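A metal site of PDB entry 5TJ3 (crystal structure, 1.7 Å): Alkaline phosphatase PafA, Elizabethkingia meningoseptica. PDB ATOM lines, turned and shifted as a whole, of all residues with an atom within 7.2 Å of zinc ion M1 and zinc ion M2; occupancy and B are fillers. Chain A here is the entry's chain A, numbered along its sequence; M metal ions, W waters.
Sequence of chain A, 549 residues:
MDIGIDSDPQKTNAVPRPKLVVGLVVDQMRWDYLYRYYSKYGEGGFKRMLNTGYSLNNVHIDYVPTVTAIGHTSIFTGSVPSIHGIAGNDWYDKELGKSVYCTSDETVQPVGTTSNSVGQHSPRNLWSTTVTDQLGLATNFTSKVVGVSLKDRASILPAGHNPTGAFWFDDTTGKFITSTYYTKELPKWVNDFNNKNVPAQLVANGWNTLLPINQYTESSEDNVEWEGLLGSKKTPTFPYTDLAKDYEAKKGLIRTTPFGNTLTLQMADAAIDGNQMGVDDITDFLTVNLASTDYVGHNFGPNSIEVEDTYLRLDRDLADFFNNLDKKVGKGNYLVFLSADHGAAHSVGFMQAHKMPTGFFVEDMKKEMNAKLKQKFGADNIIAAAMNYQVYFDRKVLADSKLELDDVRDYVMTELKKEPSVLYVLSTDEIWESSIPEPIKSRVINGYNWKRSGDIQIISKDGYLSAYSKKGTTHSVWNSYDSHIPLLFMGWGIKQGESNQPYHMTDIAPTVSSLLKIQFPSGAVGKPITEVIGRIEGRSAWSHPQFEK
Five residues have an atom within 4 Å of zinc ion M1: Asp 27, TPO 68, Asp 294, Asp 341 and His 342. Along chain A the residues within 4 Å of zinc ion M1 span positions 27 to 342.
O3P of TPO 68 binds zinc ion M2 (1.9 Å). A ring nitrogen (NE2) of His 298 is bound to zinc ion M2 (2.0 Å). Zinc ion M2 is bound by NE2 of His 475. Zinc ion M2 is bound by OD1 of Asp 294. Zinc ion M2 is bound by water W1 (2.4 Å). Slightly farther from zinc ion M2 lies the side-chain carboxylate (OD2) of Asp 294 (2.7 Å).
The side-chain carboxylate (OD1) of Asp 27 is bound to zinc ion M1, at 2.0 Å. Zinc ion M1 is bound by OG1 of TPO 68. Zinc ion M1 is bound by OD2 of Asp 341, 2.0 Å away. A ring nitrogen (NE2) of His 342 binds zinc ion M1, 2.1 Å away. Zinc ion M1 has four donor atoms within binding distance. Slightly farther from zinc ion M1 lies O3P of TPO 68 (2.8 Å).
The side-chain amide nitrogen (NE2) of Gln 28 sits at hydrogen-bond distance from the backbone carbonyl oxygen (O) of Asp 294 (3.2 Å). O of TPO 68 sits at hydrogen-bond distance from ND1 of His 72 (3.1 Å). ND1 of His 475 sits at hydrogen-bond distance from O of Thr 66, at 2.8 Å. O of Asp 27 lies within hydrogen-bond range of N of Asp 294. The side-chain carboxylate of Asp 27 is in salt-bridge range of the side-chain amino group of Lys 151 (3.0 Å). The side-chain amino group of Lys 151 is in salt-bridge range of O2P of TPO 68. The guanidinium group (NE) of Arg 153 is in salt-bridge range of O2P of TPO 68, at 3.0 Å. NZ of Lys 151 is in salt-bridge range of OD2 of Asp 294, at 2.9 Å.
Gln 28 touches zinc ion M2. Within 4 Å of zinc ion M2: Gln 28, TPO 68, Asp 294, His 298, His 342 and His 475. The nearest printed residue that does not touch zinc ion M2 is Lys 151 (4.5 Å).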
ATOM      1  N   VAL A  25      10.826 -15.080  30.361  1.00  0.00           N
ATOM      2  CA  VAL A  25       9.685 -14.212  30.132  1.00  0.00           C
ATOM      3  C   VAL A  25       8.433 -14.965  30.572  1.00  0.00           C
ATOM      4  O   VAL A  25       8.101 -16.027  30.031  1.00  0.00           O
ATOM      5  CB  VAL A  25       9.601 -13.724  28.677  1.00  0.00           C
ATOM      6  CG1 VAL A  25      10.577 -14.457  27.778  1.00  0.00           C
ATOM      7  CG2 VAL A  25       8.173 -13.708  28.140  1.00  0.00           C
ATOM      8  N   VAL A  26       7.777 -14.435  31.609  1.00  0.00           N
ATOM      9  CA  VAL A  26       6.589 -15.043  32.189  1.00  0.00           C
ATOM     10  C   VAL A  26       5.397 -14.555  31.374  1.00  0.00           C
ATOM     11  O   VAL A  26       5.070 -13.364  31.371  1.00  0.00           O
ATOM     12  CB  VAL A  26       6.425 -14.667  33.664  1.00  0.00           C
ATOM     13  CG1 VAL A  26       5.189 -15.338  34.246  1.00  0.00           C
ATOM     14  CG2 VAL A  26       7.676 -15.064  34.434  1.00  0.00           C
ATOM     15  N   ASP A  27       4.755 -15.477  30.671  1.00  0.00           N
ATOM     16  CA  ASP A  27       3.739 -15.115  29.700  1.00  0.00           C
ATOM     17  C   ASP A  27       2.523 -14.518  30.399  1.00  0.00           C
ATOM     18  O   ASP A  27       1.965 -15.113  31.325  1.00  0.00           O
ATOM     19  CB  ASP A  27       3.357 -16.347  28.885  1.00  0.00           C
ATOM     20  CG  ASP A  27       2.833 -15.995  27.526  1.00  0.00           C
ATOM     21  OD1 ASP A  27       2.027 -15.049  27.451  1.00  0.00           O
ATOM     22  OD2 ASP A  27       3.231 -16.652  26.544  1.00  0.00           O
ATOM     23  N   GLN A  28       2.130 -13.315  29.966  1.00  0.00           N
ATOM     24  CA  GLN A  28       0.968 -12.580  30.459  1.00  0.00           C
ATOM     25  C   GLN A  28       1.153 -12.052  31.879  1.00  0.00           C
ATOM     26  O   GLN A  28       0.169 -11.778  32.571  1.00  0.00           O
ATOM     27  CB  GLN A  28      -0.317 -13.430  30.388  1.00  0.00           C
ATOM     28  CG  GLN A  28      -1.586 -12.611  30.218  1.00  0.00           C
ATOM     29  CD  GLN A  28      -2.847 -13.449  30.388  1.00  0.00           C
ATOM     30  OE1 GLN A  28      -3.510 -13.364  31.425  1.00  0.00           O
ATOM     31  NE2 GLN A  28      -3.174 -14.248  29.381  1.00  0.00           N
ATOM     32  N   MET A  29       2.390 -11.895  32.345  1.00  0.00           N
ATOM     33  CA  MET A  29       2.603 -11.423  33.716  1.00  0.00           C
ATOM     34  C   MET A  29       2.481  -9.910  33.759  1.00  0.00           C
ATOM     35  O   MET A  29       3.377  -9.189  33.331  1.00  0.00           O
ATOM     36  CB  MET A  29       3.964 -11.875  34.234  1.00  0.00           C
ATOM     37  CG  MET A  29       4.185 -11.433  35.658  1.00  0.00           C
ATOM     38  SD  MET A  29       5.702 -12.090  36.366  1.00  0.00           S
ATOM     39  CE  MET A  29       5.573 -11.432  38.026  1.00  0.00           C
ATOM     40  N   THR A  66      -0.123  -6.011  21.692  1.00  0.00           N
ATOM     41  CA  THR A  66       0.657  -6.626  22.765  1.00  0.00           C
ATOM     42  C   THR A  66       0.311  -8.117  22.876  1.00  0.00           C
ATOM     43  O   THR A  66      -0.347  -8.573  23.799  1.00  0.00           O
ATOM     44  CB  THR A  66       0.445  -5.890  24.077  1.00  0.00           C
ATOM     45  OG1 THR A  66      -0.969  -5.727  24.312  1.00  0.00           O
ATOM     46  CG2 THR A  66       1.101  -4.521  24.034  1.00  0.00           C
ATOM     47  N   VAL A  67       0.792  -8.870  21.878  1.00  0.00           N
ATOM     48  CA  VAL A  67       0.603 -10.309  21.848  1.00  0.00           C
ATOM     49  C   VAL A  67       1.943 -11.040  21.989  1.00  0.00           C
ATOM     50  O   VAL A  67       2.991 -10.404  22.045  1.00  0.00           O
ATOM     51  CB  VAL A  67      -0.123 -10.743  20.566  1.00  0.00           C
ATOM     52  CG1 VAL A  67      -1.455 -10.024  20.455  1.00  0.00           C
ATOM     53  CG2 VAL A  67       0.739 -10.480  19.351  1.00  0.00           C
ATOM     54  N   TPO A  68       1.890 -12.369  22.035  1.00  0.00           N
ATOM     55  CA  TPO A  68       3.044 -13.205  22.379  1.00  0.00           C
ATOM     56  CB  TPO A  68       2.608 -14.638  22.594  1.00  0.00           C
ATOM     57  CG2 TPO A  68       3.809 -15.580  22.665  1.00  0.00           C
ATOM     58  OG1 TPO A  68       1.915 -14.706  23.821  1.00  0.00           O
ATOM     59  P   TPO A  68       0.397 -15.117  23.464  1.00  0.00           P
ATOM     60  O1P TPO A  68      -0.200 -14.166  22.491  1.00  0.00           O
ATOM     61  O2P TPO A  68       0.408 -16.594  22.831  1.00  0.00           O
ATOM     62  O3P TPO A  68      -0.425 -15.099  24.836  1.00  0.00           O
ATOM     63  C   TPO A  68       4.200 -13.159  21.392  1.00  0.00           C
ATOM     64  O   TPO A  68       5.341 -12.877  21.777  1.00  0.00           O
ATOM     65  N   ALA A  69       3.911 -13.473  20.137  1.00  0.00           N
ATOM     66  CA  ALA A  69       4.953 -13.581  19.116  1.00  0.00           C
ATOM     67  C   ALA A  69       5.765 -12.300  19.054  1.00  0.00           C
ATOM     68  O   ALA A  69       6.994 -12.347  18.982  1.00  0.00           O
ATOM     69  CB  ALA A  69       4.359 -13.907  17.765  1.00  0.00           C
ATOM     70  N   GLY A  71       5.943  -9.932  21.455  1.00  0.00           N
ATOM     71  CA  GLY A  71       6.595  -9.689  22.734  1.00  0.00           C
ATOM     72  C   GLY A  71       7.925 -10.408  22.859  1.00  0.00           C
ATOM     73  O   GLY A  71       8.938  -9.800  23.205  1.00  0.00           O
ATOM     74  N   HIS A  72       7.933 -11.704  22.561  1.00  0.00           N
ATOM     75  CA  HIS A  72       9.189 -12.452  22.624  1.00  0.00           C
ATOM     76  C   HIS A  72      10.168 -11.962  21.569  1.00  0.00           C
ATOM     77  O   HIS A  72      11.374 -11.866  21.831  1.00  0.00           O
ATOM     78  CB  HIS A  72       8.911 -13.941  22.481  1.00  0.00           C
ATOM     79  CG  HIS A  72       8.276 -14.557  23.689  1.00  0.00           C
ATOM     80  ND1 HIS A  72       6.933 -14.445  23.968  1.00  0.00           N
ATOM     81  CD2 HIS A  72       8.821 -15.234  24.725  1.00  0.00           C
ATOM     82  CE1 HIS A  72       6.670 -15.054  25.103  1.00  0.00           C
ATOM     83  NE2 HIS A  72       7.797 -15.548  25.584  1.00  0.00           N
ATOM     84  N   ASN A  89       0.919 -12.911  16.404  1.00  0.00           N
ATOM     85  CA  ASN A  89       0.889 -14.367  16.374  1.00  0.00           C
ATOM     86  C   ASN A  89       0.476 -14.866  14.991  1.00  0.00           C
ATOM     87  O   ASN A  89       0.974 -15.874  14.505  1.00  0.00           O
ATOM     88  CB  ASN A  89      -0.064 -14.913  17.430  1.00  0.00           C
ATOM     89  CG  ASN A  89       0.387 -14.591  18.842  1.00  0.00           C
ATOM     90  OD1 ASN A  89       1.569 -14.420  19.104  1.00  0.00           O
ATOM     91  ND2 ASN A  89      -0.563 -14.511  19.773  1.00  0.00           N
ATOM     92  N   LYS A 151       5.071 -23.289  24.032  1.00  0.00           N
ATOM     93  CA  LYS A 151       4.614 -22.733  22.767  1.00  0.00           C
ATOM     94  C   LYS A 151       5.766 -22.677  21.771  1.00  0.00           C
ATOM     95  O   LYS A 151       6.868 -22.237  22.112  1.00  0.00           O
ATOM     96  CB  LYS A 151       4.043 -21.324  22.939  1.00  0.00           C
ATOM     97  CG  LYS A 151       2.969 -21.160  23.987  1.00  0.00           C
ATOM     98  CD  LYS A 151       2.602 -19.685  24.099  1.00  0.00           C
ATOM     99  CE  LYS A 151       1.446 -19.458  25.050  1.00  0.00           C
ATOM    100  NZ  LYS A 151       1.007 -18.034  25.072  1.00  0.00           N
ATOM    101  N   ARG A 153       6.107 -20.612  19.208  1.00  0.00           N
ATOM    102  CA  ARG A 153       6.509 -19.225  18.940  1.00  0.00           C
ATOM    103  C   ARG A 153       7.386 -18.678  20.055  1.00  0.00           C
ATOM    104  O   ARG A 153       8.324 -17.909  19.797  1.00  0.00           O
ATOM    105  CB  ARG A 153       5.277 -18.352  18.738  1.00  0.00           C
ATOM    106  CG  ARG A 153       4.231 -18.424  19.853  1.00  0.00           C
ATOM    107  CD  ARG A 153       2.989 -17.624  19.481  1.00  0.00           C
ATOM    108  NE  ARG A 153       1.946 -17.658  20.502  1.00  0.00           N
ATOM    109  CZ  ARG A 153       0.991 -18.581  20.549  1.00  0.00           C
ATOM    110  NH1 ARG A 153       0.945 -19.547  19.650  1.00  0.00           N
ATOM    111  NH2 ARG A 153       0.073 -18.535  21.515  1.00  0.00           N
ATOM    112  N   ALA A 154       7.105 -19.049  21.298  1.00  0.00           N
ATOM    113  CA  ALA A 154       7.830 -18.506  22.445  1.00  0.00           C
ATOM    114  C   ALA A 154       9.171 -19.204  22.685  1.00  0.00           C
ATOM    115  O   ALA A 154       9.945 -18.737  23.536  1.00  0.00           O
ATOM    116  CB  ALA A 154       6.968 -18.596  23.701  1.00  0.00           C
ATOM    117  N   ASN A 289      10.376 -19.456  28.154  1.00  0.00           N
ATOM    118  CA  ASN A 289       9.090 -18.799  28.334  1.00  0.00           C
ATOM    119  C   ASN A 289       8.230 -19.658  29.236  1.00  0.00           C
ATOM    120  O   ASN A 289       8.113 -20.870  29.020  1.00  0.00           O
ATOM    121  CB  ASN A 289       8.410 -18.583  26.983  1.00  0.00           C
ATOM    122  CG  ASN A 289       6.895 -18.557  27.092  1.00  0.00           C
ATOM    123  OD1 ASN A 289       6.239 -19.595  26.997  1.00  0.00           O
ATOM    124  ND2 ASN A 289       6.342 -17.374  27.280  1.00  0.00           N
ATOM    125  N   ALA A 291       4.728 -20.380  29.901  1.00  0.00           N
ATOM    126  CA  ALA A 291       3.507 -20.129  29.158  1.00  0.00           C
ATOM    127  C   ALA A 291       2.232 -20.342  29.968  1.00  0.00           C
ATOM    128  O   ALA A 291       1.182 -19.787  29.599  1.00  0.00           O
ATOM    129  CB  ALA A 291       3.453 -21.001  27.908  1.00  0.00           C
ATOM    130  N   ASP A 294      -0.115 -17.648  31.059  1.00  0.00           N
ATOM    131  CA  ASP A 294      -0.960 -17.093  30.000  1.00  0.00           C
ATOM    132  C   ASP A 294      -2.192 -17.946  29.758  1.00  0.00           C
ATOM    133  O   ASP A 294      -3.297 -17.427  29.618  1.00  0.00           O
ATOM    134  CB  ASP A 294      -0.150 -16.965  28.711  1.00  0.00           C
ATOM    135  CG  ASP A 294      -0.947 -16.390  27.572  1.00  0.00           C
ATOM    136  OD1 ASP A 294      -1.215 -15.167  27.591  1.00  0.00           O
ATOM    137  OD2 ASP A 294      -1.307 -17.161  26.652  1.00  0.00           O
ATOM    138  N   TYR A 295      -2.012 -19.266  29.693  1.00  0.00           N
ATOM    139  CA  TYR A 295      -3.152 -20.163  29.505  1.00  0.00           C
ATOM    140  C   TYR A 295      -4.107 -20.056  30.685  1.00  0.00           C
ATOM    141  O   TYR A 295      -5.326 -19.925  30.502  1.00  0.00           O
ATOM    142  CB  TYR A 295      -2.670 -21.598  29.319  1.00  0.00           C
ATOM    143  CG  TYR A 295      -2.063 -21.843  27.964  1.00  0.00           C
ATOM    144  CD1 TYR A 295      -2.860 -21.997  26.842  1.00  0.00           C
ATOM    145  CD2 TYR A 295      -0.685 -21.927  27.798  1.00  0.00           C
ATOM    146  CE1 TYR A 295      -2.311 -22.220  25.590  1.00  0.00           C
ATOM    147  CE2 TYR A 295      -0.117 -22.153  26.557  1.00  0.00           C
ATOM    148  CZ  TYR A 295      -0.946 -22.301  25.458  1.00  0.00           C
ATOM    149  OH  TYR A 295      -0.406 -22.522  24.212  1.00  0.00           O
ATOM    150  N   HIS A 298      -5.784 -16.610  30.581  1.00  0.00           N
ATOM    151  CA  HIS A 298      -6.779 -16.527  29.520  1.00  0.00           C
ATOM    152  C   HIS A 298      -8.101 -17.156  29.934  1.00  0.00           C
ATOM    153  O   HIS A 298      -9.177 -16.689  29.550  1.00  0.00           O
ATOM    154  CB  HIS A 298      -6.259 -17.201  28.258  1.00  0.00           C
ATOM    155  CG  HIS A 298      -5.517 -16.282  27.333  1.00  0.00           C
ATOM    156  ND1 HIS A 298      -6.142 -15.259  26.654  1.00  0.00           N
ATOM    157  CD2 HIS A 298      -4.215 -16.247  26.975  1.00  0.00           C
ATOM    158  CE1 HIS A 298      -5.242 -14.626  25.922  1.00  0.00           C
ATOM    159  NE2 HIS A 298      -4.073 -15.205  26.098  1.00  0.00           N
ATOM    160  N   ALA A 340       8.043  -9.952  30.847  1.00  0.00           N
ATOM    161  CA  ALA A 340       6.836 -10.542  30.309  1.00  0.00           C
ATOM    162  C   ALA A 340       6.646 -10.035  28.891  1.00  0.00           C
ATOM    163  O   ALA A 340       7.151  -8.972  28.521  1.00  0.00           O
ATOM    164  CB  ALA A 340       5.609 -10.193  31.163  1.00  0.00           C
ATOM    165  N   ASP A 341       5.936 -10.815  28.090  1.00  0.00           N
ATOM    166  CA  ASP A 341       5.645 -10.381  26.723  1.00  0.00           C
ATOM    167  C   ASP A 341       4.457  -9.442  26.655  1.00  0.00           C
ATOM    168  O   ASP A 341       4.258  -8.803  25.610  1.00  0.00           O
ATOM    169  CB  ASP A 341       5.418 -11.601  25.827  1.00  0.00           C
ATOM    170  CG  ASP A 341       4.380 -12.559  26.380  1.00  0.00           C
ATOM    171  OD1 ASP A 341       4.038 -12.474  27.573  1.00  0.00           O
ATOM    172  OD2 ASP A 341       3.920 -13.422  25.604  1.00  0.00           O
ATOM    173  N   HIS A 342       3.688  -9.327  27.744  1.00  0.00           N
ATOM    174  CA  HIS A 342       2.538  -8.441  27.865  1.00  0.00           C
ATOM    175  C   HIS A 342       1.861  -8.671  29.211  1.00  0.00           C
ATOM    176  O   HIS A 342       2.187  -9.623  29.921  1.00  0.00           O
ATOM    177  CB  HIS A 342       1.526  -8.701  26.747  1.00  0.00           C
ATOM    178  CG  HIS A 342       1.161 -10.144  26.607  1.00  0.00           C
ATOM    179  ND1 HIS A 342       0.330 -10.784  27.510  1.00  0.00           N
ATOM    180  CD2 HIS A 342       1.546 -11.091  25.717  1.00  0.00           C
ATOM    181  CE1 HIS A 342       0.208 -12.050  27.159  1.00  0.00           C
ATOM    182  NE2 HIS A 342       0.939 -12.259  26.075  1.00  0.00           N
ATOM    183  N   GLY A 343       0.934  -7.796  29.579  1.00  0.00           N
ATOM    184  CA  GLY A 343       0.079  -7.991  30.734  1.00  0.00           C
ATOM    185  C   GLY A 343      -1.242  -8.618  30.343  1.00  0.00           C
ATOM    186  O   GLY A 343      -1.309  -9.459  29.434  1.00  0.00           O
ATOM    187  N   THR A 473      -9.873 -13.730  30.051  1.00  0.00           N
ATOM    188  CA  THR A 473      -9.396 -12.410  29.627  1.00  0.00           C
ATOM    189  C   THR A 473      -8.495 -12.580  28.406  1.00  0.00           C
ATOM    190  O   THR A 473      -8.256 -13.686  27.930  1.00  0.00           O
ATOM    191  CB  THR A 473      -8.677 -11.684  30.771  1.00  0.00           C
ATOM    192  OG1 THR A 473      -8.526 -10.307  30.431  1.00  0.00           O
ATOM    193  CG2 THR A 473      -7.301 -12.307  31.006  1.00  0.00           C
ATOM    194  N   THR A 474      -8.006 -11.446  27.907  1.00  0.00           N
ATOM    195  CA  THR A 474      -7.109 -11.431  26.754  1.00  0.00           C
ATOM    196  C   THR A 474      -6.271 -10.161  26.819  1.00  0.00           C
ATOM    197  O   THR A 474      -6.337  -9.398  27.789  1.00  0.00           O
ATOM    198  CB  THR A 474      -7.895 -11.551  25.445  1.00  0.00           C
ATOM    199  OG1 THR A 474      -6.994 -11.749  24.354  1.00  0.00           O
ATOM    200  CG2 THR A 474      -8.714 -10.292  25.202  1.00  0.00           C
ATOM    201  N   HIS A 475      -5.500  -9.920  25.762  1.00  0.00           N
ATOM    202  CA  HIS A 475      -4.472  -8.886  25.772  1.00  0.00           C
ATOM    203  C   HIS A 475      -4.102  -8.545  24.331  1.00  0.00           C
ATOM    204  O   HIS A 475      -3.929  -9.455  23.517  1.00  0.00           O
ATOM    205  CB  HIS A 475      -3.237  -9.403  26.516  1.00  0.00           C
ATOM    206  CG  HIS A 475      -2.696 -10.664  25.928  1.00  0.00           C
ATOM    207  ND1 HIS A 475      -1.897 -10.682  24.803  1.00  0.00           N
ATOM    208  CD2 HIS A 475      -2.893 -11.962  26.271  1.00  0.00           C
ATOM    209  CE1 HIS A 475      -1.588 -11.928  24.498  1.00  0.00           C
ATOM    210  NE2 HIS A 475      -2.184 -12.721  25.370  1.00  0.00           N
HETATM  211 ZN    ZN M   1       1.996 -14.068  25.749  1.00  0.00          ZN
HETATM  212 ZN    ZN M   2      -2.126 -14.866  25.592  1.00  0.00          ZN
HETATM  213  O   HOH W   1      -2.680 -15.564  23.326  1.00  0.00           O
